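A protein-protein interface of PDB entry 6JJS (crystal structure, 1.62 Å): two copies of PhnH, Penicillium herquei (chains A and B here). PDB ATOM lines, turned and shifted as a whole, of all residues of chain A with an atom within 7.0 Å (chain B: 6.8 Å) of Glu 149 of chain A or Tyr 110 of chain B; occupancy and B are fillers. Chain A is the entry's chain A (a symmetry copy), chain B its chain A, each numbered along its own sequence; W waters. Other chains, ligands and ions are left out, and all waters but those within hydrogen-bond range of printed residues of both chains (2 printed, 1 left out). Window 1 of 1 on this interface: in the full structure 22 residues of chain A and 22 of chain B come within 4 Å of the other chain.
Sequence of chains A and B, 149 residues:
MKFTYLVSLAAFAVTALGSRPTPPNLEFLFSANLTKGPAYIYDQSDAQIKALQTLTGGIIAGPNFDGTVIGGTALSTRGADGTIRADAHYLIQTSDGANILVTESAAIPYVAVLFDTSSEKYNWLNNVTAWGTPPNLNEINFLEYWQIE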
ATOM      1  N   PRO A  23      -0.653 -16.253   4.334  1.00  0.00           N
ATOM      2  CA  PRO A  23      -1.344 -15.005   4.027  1.00  0.00           C
ATOM      3  C   PRO A  23      -2.273 -14.598   5.155  1.00  0.00           C
ATOM      4  O   PRO A  23      -2.749 -15.428   5.926  1.00  0.00           O
ATOM      5  CB  PRO A  23      -2.137 -15.333   2.760  1.00  0.00           C
ATOM      6  CG  PRO A  23      -2.364 -16.819   2.852  1.00  0.00           C
ATOM      7  CD  PRO A  23      -1.103 -17.364   3.489  1.00  0.00           C
ATOM      8  N   PRO A  24      -2.577 -13.293   5.273  1.00  0.00           N
ATOM      9  CA  PRO A  24      -3.569 -12.820   6.228  1.00  0.00           C
ATOM     10  C   PRO A  24      -4.982 -13.243   5.815  1.00  0.00           C
ATOM     11  O   PRO A  24      -5.189 -13.661   4.690  1.00  0.00           O
ATOM     12  CB  PRO A  24      -3.436 -11.292   6.149  1.00  0.00           C
ATOM     13  CG  PRO A  24      -2.975 -11.061   4.743  1.00  0.00           C
ATOM     14  CD  PRO A  24      -2.032 -12.209   4.440  1.00  0.00           C
ATOM     15  N   ASN A  25      -5.886 -13.176   6.781  1.00  0.00           N
ATOM     16  CA  ASN A  25      -7.326 -13.437   6.600  1.00  0.00           C
ATOM     17  C   ASN A  25      -7.986 -12.113   6.258  1.00  0.00           C
ATOM     18  O   ASN A  25      -7.428 -11.030   6.639  1.00  0.00           O
ATOM     19  CB  ASN A  25      -7.932 -14.133   7.822  1.00  0.00           C
ATOM     20  CG  ASN A  25      -7.558 -15.603   7.868  1.00  0.00           C
ATOM     21  OD1 ASN A  25      -7.797 -16.337   6.914  1.00  0.00           O
ATOM     22  ND2 ASN A  25      -6.896 -16.025   8.930  1.00  0.00           N
ATOM     23  N   LEU A  26      -9.046 -12.204   5.465  1.00  0.00           N
ATOM     24  CA  LEU A  26      -9.834 -11.066   4.950  1.00  0.00           C
ATOM     25  C   LEU A  26     -11.259 -11.224   5.470  1.00  0.00           C
ATOM     26  O   LEU A  26     -11.841 -12.309   5.265  1.00  0.00           O
ATOM     27  CB  LEU A  26      -9.812 -11.104   3.423  1.00  0.00           C
ATOM     28  CG  LEU A  26      -8.420 -11.058   2.804  1.00  0.00           C
ATOM     29  CD1 LEU A  26      -8.478 -11.420   1.325  1.00  0.00           C
ATOM     30  CD2 LEU A  26      -7.807  -9.683   3.002  1.00  0.00           C
ATOM     31  N   GLU A  27     -11.802 -10.216   6.134  1.00  0.00           N
ATOM     32  CA  GLU A  27     -13.219 -10.249   6.567  1.00  0.00           C
ATOM     33  C   GLU A  27     -13.917  -8.982   6.081  1.00  0.00           C
ATOM     34  O   GLU A  27     -13.359  -7.876   6.237  1.00  0.00           O
ATOM     35  CB  GLU A  27     -13.304 -10.416   8.082  1.00  0.00           C
ATOM     36  CG  GLU A  27     -14.690 -10.785   8.568  1.00  0.00           C
ATOM     37  CD  GLU A  27     -14.839 -10.770  10.081  1.00  0.00           C
ATOM     38  OE1 GLU A  27     -15.989 -10.664  10.560  1.00  0.00           O
ATOM     39  OE2 GLU A  27     -13.804 -10.869  10.779  1.00  0.00           O
ATOM     40  N   LEU A 114      -7.028   3.267   7.913  1.00  0.00           N
ATOM     41  CA  LEU A 114      -6.917   3.223   9.381  1.00  0.00           C
ATOM     42  C   LEU A 114      -8.082   3.994   9.999  1.00  0.00           C
ATOM     43  O   LEU A 114      -8.681   4.837   9.313  1.00  0.00           O
ATOM     44  CB  LEU A 114      -5.557   3.805   9.808  1.00  0.00           C
ATOM     45  CG  LEU A 114      -4.345   3.004   9.347  1.00  0.00           C
ATOM     46  CD1 LEU A 114      -3.071   3.824   9.479  1.00  0.00           C
ATOM     47  CD2 LEU A 114      -4.208   1.703  10.111  1.00  0.00           C
ATOM     48  N   TRP A 124     -12.409  -1.260  18.856  1.00  0.00           N
ATOM     49  CA  TRP A 124     -11.670  -2.364  18.199  1.00  0.00           C
ATOM     50  C   TRP A 124     -11.135  -1.874  16.844  1.00  0.00           C
ATOM     51  O   TRP A 124     -10.078  -2.357  16.440  1.00  0.00           O
ATOM     52  CB  TRP A 124     -12.572  -3.598  18.069  1.00  0.00           C
ATOM     53  CG  TRP A 124     -13.845  -3.368  17.315  1.00  0.00           C
ATOM     54  CD1 TRP A 124     -15.048  -2.907  17.777  1.00  0.00           C
ATOM     55  CD2 TRP A 124     -14.054  -3.711  15.936  1.00  0.00           C
ATOM     56  NE1 TRP A 124     -15.976  -2.898  16.761  1.00  0.00           N
ATOM     57  CE2 TRP A 124     -15.393  -3.395  15.624  1.00  0.00           C
ATOM     58  CE3 TRP A 124     -13.220  -4.232  14.941  1.00  0.00           C
ATOM     59  CZ2 TRP A 124     -15.919  -3.590  14.351  1.00  0.00           C
ATOM     60  CZ3 TRP A 124     -13.746  -4.440  13.688  1.00  0.00           C
ATOM     61  CH2 TRP A 124     -15.074  -4.115  13.399  1.00  0.00           C
ATOM     62  N   ASN A 127      -7.407  -0.833  16.182  1.00  0.00           N
ATOM     63  CA  ASN A 127      -6.404  -1.892  15.967  1.00  0.00           C
ATOM     64  C   ASN A 127      -6.531  -2.501  14.565  1.00  0.00           C
ATOM     65  O   ASN A 127      -5.827  -3.500  14.312  1.00  0.00           O
ATOM     66  CB  ASN A 127      -6.509  -2.989  17.025  1.00  0.00           C
ATOM     67  CG  ASN A 127      -6.114  -2.487  18.390  1.00  0.00           C
ATOM     68  OD1 ASN A 127      -5.097  -1.811  18.516  1.00  0.00           O
ATOM     69  ND2 ASN A 127      -6.994  -2.671  19.367  1.00  0.00           N
ATOM     70  N   VAL A 128      -7.358  -1.929  13.691  1.00  0.00           N
ATOM     71  CA  VAL A 128      -7.682  -2.533  12.369  1.00  0.00           C
ATOM     72  C   VAL A 128      -6.928  -1.810  11.245  1.00  0.00           C
ATOM     73  O   VAL A 128      -6.988  -0.575  11.165  1.00  0.00           O
ATOM     74  CB  VAL A 128      -9.189  -2.526  12.113  1.00  0.00           C
ATOM     75  CG1 VAL A 128      -9.524  -2.941  10.683  1.00  0.00           C
ATOM     76  CG2 VAL A 128      -9.872  -3.434  13.122  1.00  0.00           C
ATOM     77  N   THR A 129      -6.317  -2.601  10.363  1.00  0.00           N
ATOM     78  CA  THR A 129      -5.959  -2.177   8.989  1.00  0.00           C
ATOM     79  C   THR A 129      -7.019  -2.717   8.038  1.00  0.00           C
ATOM     80  O   THR A 129      -7.244  -3.956   8.032  1.00  0.00           O
ATOM     81  CB  THR A 129      -4.590  -2.708   8.584  1.00  0.00           C
ATOM     82  OG1 THR A 129      -4.602  -4.115   8.851  1.00  0.00           O
ATOM     83  CG2 THR A 129      -3.461  -2.036   9.331  1.00  0.00           C
ATOM     84  N   GLN A 147     -11.334  -6.017   6.447  1.00  0.00           N
ATOM     85  CA  GLN A 147     -10.359  -6.099   7.559  1.00  0.00           C
ATOM     86  C   GLN A 147      -9.297  -7.117   7.146  1.00  0.00           C
ATOM     87  O   GLN A 147      -9.650  -8.263   6.818  1.00  0.00           O
ATOM     88  CB  GLN A 147     -11.086  -6.464   8.853  1.00  0.00           C
ATOM     89  CG  GLN A 147     -10.175  -6.738  10.032  1.00  0.00           C
ATOM     90  CD  GLN A 147     -10.997  -6.934  11.286  1.00  0.00           C
ATOM     91  OE1 GLN A 147     -12.217  -6.820  11.273  1.00  0.00           O
ATOM     92  NE2 GLN A 147     -10.319  -7.023  12.410  1.00  0.00           N
ATOM     93  N   ILE A 148      -8.035  -6.710   7.176  1.00  0.00           N
ATOM     94  CA  ILE A 148      -6.871  -7.587   6.896  1.00  0.00           C
ATOM     95  C   ILE A 148      -6.139  -7.863   8.209  1.00  0.00           C
ATOM     96  O   ILE A 148      -5.735  -6.883   8.870  1.00  0.00           O
ATOM     97  CB  ILE A 148      -5.930  -6.957   5.861  1.00  0.00           C
ATOM     98  CG1 ILE A 148      -6.690  -6.398   4.657  1.00  0.00           C
ATOM     99  CG2 ILE A 148      -4.882  -7.992   5.458  1.00  0.00           C
ATOM    100  CD1 ILE A 148      -5.785  -5.945   3.542  1.00  0.00           C
ATOM    101  N   GLU A 149      -6.046  -9.135   8.607  1.00  0.00           N
ATOM    102  CA  GLU A 149      -5.235  -9.542   9.781  1.00  0.00           C
ATOM    103  C   GLU A 149      -4.960 -11.043   9.763  1.00  0.00           C
ATOM    104  O   GLU A 149      -5.498 -11.803   8.994  1.00  0.00           O
ATOM    105  CB  GLU A 149      -5.838  -9.155  11.125  1.00  0.00           C
ATOM    106  CG  GLU A 149      -7.333  -9.148  11.209  1.00  0.00           C
ATOM    107  CD  GLU A 149      -7.747  -8.625  12.573  1.00  0.00           C
ATOM    108  OE1 GLU A 149      -7.714  -7.361  12.772  1.00  0.00           O
ATOM    109  OE2 GLU A 149      -7.934  -9.470  13.474  1.00  0.00           O
ATOM    110  OXT GLU A 149      -4.154 -11.451  10.584  1.00  0.00           O
ATOM    111  N   ILE B  84      -1.054   0.530  19.403  1.00  0.00           N
ATOM    112  CA  ILE B  84       0.171   1.193  18.902  1.00  0.00           C
ATOM    113  C   ILE B  84      -0.074   1.606  17.454  1.00  0.00           C
ATOM    114  O   ILE B  84      -0.397   0.737  16.619  1.00  0.00           O
ATOM    115  CB  ILE B  84       1.382   0.263  19.019  1.00  0.00           C
ATOM    116  CG1 ILE B  84       1.598  -0.228  20.453  1.00  0.00           C
ATOM    117  CG2 ILE B  84       2.599   0.951  18.431  1.00  0.00           C
ATOM    118  CD1 ILE B  84       2.660  -1.310  20.566  1.00  0.00           C
ATOM    119  N   SER B 105       2.256   2.717   7.262  1.00  0.00           N
ATOM    120  CA  SER B 105       1.296   3.189   8.288  1.00  0.00           C
ATOM    121  C   SER B 105       0.705   1.943   8.935  1.00  0.00           C
ATOM    122  O   SER B 105       0.289   1.022   8.210  1.00  0.00           O
ATOM    123  CB  SER B 105       0.285   4.124   7.710  1.00  0.00           C
ATOM    124  OG  SER B 105      -0.292   3.593   6.560  1.00  0.00           O
ATOM    125  N   ALA B 106       0.739   1.891  10.257  1.00  0.00           N
ATOM    126  CA  ALA B 106       0.496   0.633  10.974  1.00  0.00           C
ATOM    127  C   ALA B 106      -0.472   0.839  12.123  1.00  0.00           C
ATOM    128  O   ALA B 106      -0.330   1.802  12.909  1.00  0.00           O
ATOM    129  CB  ALA B 106       1.810   0.096  11.466  1.00  0.00           C
ATOM    130  N   ALA B 107      -1.303  -0.167  12.317  1.00  0.00           N
ATOM    131  CA  ALA B 107      -1.982  -0.461  13.598  1.00  0.00           C
ATOM    132  C   ALA B 107      -1.309  -1.712  14.137  1.00  0.00           C
ATOM    133  O   ALA B 107      -1.651  -2.816  13.699  1.00  0.00           O
ATOM    134  CB  ALA B 107      -3.462  -0.658  13.381  1.00  0.00           C
ATOM    135  N   ILE B 108      -0.217  -1.502  14.847  1.00  0.00           N
ATOM    136  CA  ILE B 108       0.776  -2.578  15.115  1.00  0.00           C
ATOM    137  C   ILE B 108       0.022  -3.756  15.720  1.00  0.00           C
ATOM    138  O   ILE B 108      -0.835  -3.557  16.584  1.00  0.00           O
ATOM    139  CB  ILE B 108       1.839  -2.026  16.067  1.00  0.00           C
ATOM    140  CG1 ILE B 108       2.740  -1.005  15.369  1.00  0.00           C
ATOM    141  CG2 ILE B 108       2.603  -3.161  16.731  1.00  0.00           C
ATOM    142  CD1 ILE B 108       3.511  -1.547  14.240  1.00  0.00           C
ATOM    143  N   PRO B 109       0.241  -5.009  15.264  1.00  0.00           N
ATOM    144  CA  PRO B 109       1.351  -5.401  14.395  1.00  0.00           C
ATOM    145  C   PRO B 109       1.065  -5.476  12.892  1.00  0.00           C
ATOM    146  O   PRO B 109       1.840  -6.069  12.150  1.00  0.00           O
ATOM    147  CB  PRO B 109       1.637  -6.837  14.869  1.00  0.00           C
ATOM    148  CG  PRO B 109       0.240  -7.374  15.216  1.00  0.00           C
ATOM    149  CD  PRO B 109      -0.522  -6.177  15.747  1.00  0.00           C
ATOM    150  N   TYR B 110      -0.023  -4.832  12.458  1.00  0.00           N
ATOM    151  CA  TYR B 110      -0.494  -4.836  11.059  1.00  0.00           C
ATOM    152  C   TYR B 110       0.045  -3.594  10.347  1.00  0.00           C
ATOM    153  O   TYR B 110      -0.218  -2.487  10.802  1.00  0.00           O
ATOM    154  CB  TYR B 110      -2.016  -4.909  11.043  1.00  0.00           C
ATOM    155  CG  TYR B 110      -2.578  -5.984  11.933  1.00  0.00           C
ATOM    156  CD1 TYR B 110      -2.108  -7.288  11.871  1.00  0.00           C
ATOM    157  CD2 TYR B 110      -3.569  -5.675  12.840  1.00  0.00           C
ATOM    158  CE1 TYR B 110      -2.619  -8.259  12.722  1.00  0.00           C
ATOM    159  CE2 TYR B 110      -4.105  -6.643  13.672  1.00  0.00           C
ATOM    160  CZ  TYR B 110      -3.616  -7.929  13.615  1.00  0.00           C
ATOM    161  OH  TYR B 110      -4.179  -8.863  14.446  1.00  0.00           O
ATOM    162  N   VAL B 111       0.718  -3.786   9.216  1.00  0.00           N
ATOM    163  CA  VAL B 111       1.457  -2.695   8.542  1.00  0.00           C
ATOM    164  C   VAL B 111       0.966  -2.538   7.114  1.00  0.00           C
ATOM    165  O   VAL B 111       1.144  -3.473   6.308  1.00  0.00           O
ATOM    166  CB  VAL B 111       2.962  -2.946   8.578  1.00  0.00           C
ATOM    167  CG1 VAL B 111       3.694  -1.733   8.022  1.00  0.00           C
ATOM    168  CG2 VAL B 111       3.426  -3.287   9.980  1.00  0.00           C
ATOM    169  N   ALA B 112       0.443  -1.355   6.790  1.00  0.00           N
ATOM    170  CA  ALA B 112       0.064  -1.006   5.401  1.00  0.00           C
ATOM    171  C   ALA B 112       1.233  -0.289   4.719  1.00  0.00           C
ATOM    172  O   ALA B 112       1.953   0.478   5.381  1.00  0.00           O
ATOM    173  CB  ALA B 112      -1.176  -0.152   5.375  1.00  0.00           C
ATOM    174  N   TRP B 131       0.720  -5.073   2.424  1.00  0.00           N
ATOM    175  CA  TRP B 131       0.318  -5.265   3.829  1.00  0.00           C
ATOM    176  C   TRP B 131       1.234  -6.320   4.414  1.00  0.00           C
ATOM    177  O   TRP B 131       1.514  -7.316   3.721  1.00  0.00           O
ATOM    178  CB  TRP B 131      -1.146  -5.697   3.893  1.00  0.00           C
ATOM    179  CG  TRP B 131      -1.671  -5.866   5.279  1.00  0.00           C
ATOM    180  CD1 TRP B 131      -2.453  -4.977   5.951  1.00  0.00           C
ATOM    181  CD2 TRP B 131      -1.442  -6.963   6.183  1.00  0.00           C
ATOM    182  NE1 TRP B 131      -2.746  -5.442   7.199  1.00  0.00           N
ATOM    183  CE2 TRP B 131      -2.192  -6.688   7.351  1.00  0.00           C
ATOM    184  CE3 TRP B 131      -0.799  -8.204   6.073  1.00  0.00           C
ATOM    185  CZ2 TRP B 131      -2.241  -7.558   8.437  1.00  0.00           C
ATOM    186  CZ3 TRP B 131      -0.896  -9.080   7.124  1.00  0.00           C
ATOM    187  CH2 TRP B 131      -1.565  -8.748   8.301  1.00  0.00           C
ATOM    188  N   GLY B 132       1.720  -6.078   5.612  1.00  0.00           N
ATOM    189  CA  GLY B 132       2.639  -7.022   6.263  1.00  0.00           C
ATOM    190  C   GLY B 132       2.421  -7.116   7.745  1.00  0.00           C
ATOM    191  O   GLY B 132       1.793  -6.241   8.377  1.00  0.00           O
ATOM    192  N   THR B 133       3.015  -8.155   8.316  1.00  0.00           N
ATOM    193  CA  THR B 133       2.971  -8.430   9.761  1.00  0.00           C
ATOM    194  C   THR B 133       4.124  -9.385  10.050  1.00  0.00           C
ATOM    195  O   THR B 133       4.529 -10.135   9.163  1.00  0.00           O
ATOM    196  CB  THR B 133       1.585  -8.947  10.180  1.00  0.00           C
ATOM    197  OG1 THR B 133       1.483  -8.768  11.595  1.00  0.00           O
ATOM    198  CG2 THR B 133       1.357 -10.401   9.817  1.00  0.00           C
ATOM    199  N   PRO B 134       4.675  -9.382  11.283  1.00  0.00           N
ATOM    200  CA  PRO B 134       5.702 -10.363  11.634  1.00  0.00           C
ATOM    201  C   PRO B 134       5.013 -11.717  11.707  1.00  0.00           C
ATOM    202  O   PRO B 134       4.009 -11.874  12.423  1.00  0.00           O
ATOM    203  CB  PRO B 134       6.196  -9.906  13.003  1.00  0.00           C
ATOM    204  CG  PRO B 134       5.720  -8.462  13.133  1.00  0.00           C
ATOM    205  CD  PRO B 134       4.418  -8.432  12.369  1.00  0.00           C
ATOM    206  N   LEU B 137       5.424 -13.084  16.307  1.00  0.00           N
ATOM    207  CA  LEU B 137       5.278 -11.836  17.081  1.00  0.00           C
ATOM    208  C   LEU B 137       6.313 -11.728  18.193  1.00  0.00           C
ATOM    209  O   LEU B 137       6.370 -10.697  18.850  1.00  0.00           O
ATOM    210  CB  LEU B 137       3.843 -11.691  17.579  1.00  0.00           C
ATOM    211  CG  LEU B 137       2.836 -11.443  16.460  1.00  0.00           C
ATOM    212  CD1 LEU B 137       1.408 -11.553  16.969  1.00  0.00           C
ATOM    213  CD2 LEU B 137       3.069 -10.080  15.813  1.00  0.00           C
ATOM    214  N   LEU B 143       9.300  -9.094   9.024  1.00  0.00           N
ATOM    215  CA  LEU B 143       7.919  -8.989   8.490  1.00  0.00           C
ATOM    216  C   LEU B 143       7.836  -9.607   7.110  1.00  0.00           C
ATOM    217  O   LEU B 143       8.809  -9.519   6.322  1.00  0.00           O
ATOM    218  CB  LEU B 143       7.482  -7.528   8.453  1.00  0.00           C
ATOM    219  CG  LEU B 143       7.442  -6.816   9.800  1.00  0.00           C
ATOM    220  CD1 LEU B 143       8.771  -6.112  10.049  1.00  0.00           C
ATOM    221  CD2 LEU B 143       6.281  -5.839   9.830  1.00  0.00           C
HETATM  222  O   HOH W   1      -4.353 -11.361  13.687  1.00  0.00           O
HETATM  223  O   HOH W   2      -2.497  -1.397  17.630  1.00  0.00           O
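NE1 of Trp 131 of chain B sits at hydrogen-bond distance from OG1 of Thr 129 of chain A, 2.8 Å away.
Pro 24 of chain A touches Trp 131 of chain B.
CD1 of Leu 114 of chain A touches CB of Ser 105 of chain B, 3.8 Å away.
CB of Ala 107 of chain B touches C of Asn 127 of chain A, at 3.8 Å.
Asn 127 of chain A touches Tyr 110 of chain B (O to CD2, 3.5 Å).
CB of Tyr 110 of chain B touches OG1 of Thr 129 of chain A, at 3.5 Å.
CE2 of Trp 131 of chain B touches CG2 of Ile 148 of chain A (3.5 Å).
CZ of Tyr 110 of chain B touches CB of Glu 149 of chain A (3.6 Å).
CA of Glu 149 of chain A touches CZ2 of Trp 131 of chain B (3.8 Å).
No position is printed for both chains.
Of the 9 pairs that touch across the chains among the printed residues, none has its exchanged pair printed and touching as well.
The backbone NH (N) of Asn 25 of chain A lies within hydrogen-bond range of the chain-end carboxylate (O) of Glu 149 of chain A.
The backbone carbonyl oxygen (O) of Ser 105 of chain B is in hydrogen-bond range of the backbone NH (N) of Ala 112 of chain B, at 2.8 Å.
OE1 of Glu 149 of chain A sits at hydrogen-bond distance from NE2 of Gln 147 of chain A (2.7 Å).
The backbone NH (N) of Ile 148 of chain A is in hydrogen-bond range of the backbone carbonyl oxygen (O) of Thr 129 of chain A (3.0 Å).
Printed residues of chain B that touch a printed residue of chain A: Ser 105, Ala 107, Tyr 110 and Trp 131.
Hydrophobic or aromatic side chains of chain B that line the printed part of chain A: Ala 107, Tyr 110 and Trp 131.
Printed residues of chain A that touch a printed residue of chain B: Pro 24, Leu 114, Asn 127, Thr 129, Ile 148 and Glu 149.
Tyr 110 of chain B touches just these residues of chain A: Asn 127 (3.5 Å), Thr 129 (3.5 Å) and Glu 149 (3.6 Å).
Printed residues of chain B within 4 Å of Leu 114 of chain A: Ser 105.
Of the printed residues of chain A, Trp 131 of chain B touches Pro 24, Thr 129, Ile 148 and Glu 149.
Printed residues of chain B within 4 Å of Pro 24 of chain A: Trp 131 (3.5 Å).
Of the printed residues of chain B, Ile 148 of chain A touches Trp 131.
Pro 23 of chain A touches none of the printed residues of chain B.
Val 128 of chain A touches none of the printed residues of chain B.
The nearest residue of chain B that does not touch Glu 149 of chain A is Thr 133 of chain B (5.7 Å).
The nearest residue of chain A that does not touch Tyr 110 of chain B is Ile 148 of chain A (4.5 Å).
The nearest printed residue of chain A that does not touch Ala 107 of chain B is Leu 114 of chain A (4.1 Å).
Water W1 lies within hydrogen-bond range of the side-chain hydroxyl (OH) of Tyr 110 of chain B (2.6 Å) and the chain-end carboxylate (OXT) of Glu 149 of chain A (3.1 Å).
Water W2 lies within hydrogen-bond range of the side-chain amide oxygen (OD1) of Asn 127 of chain A (2.8 Å), the backbone carbonyl oxygen (O) of Ile 108 of chain B (2.9 Å) and the backbone NH (N) of Ile 84 of chain B (3.0 Å).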
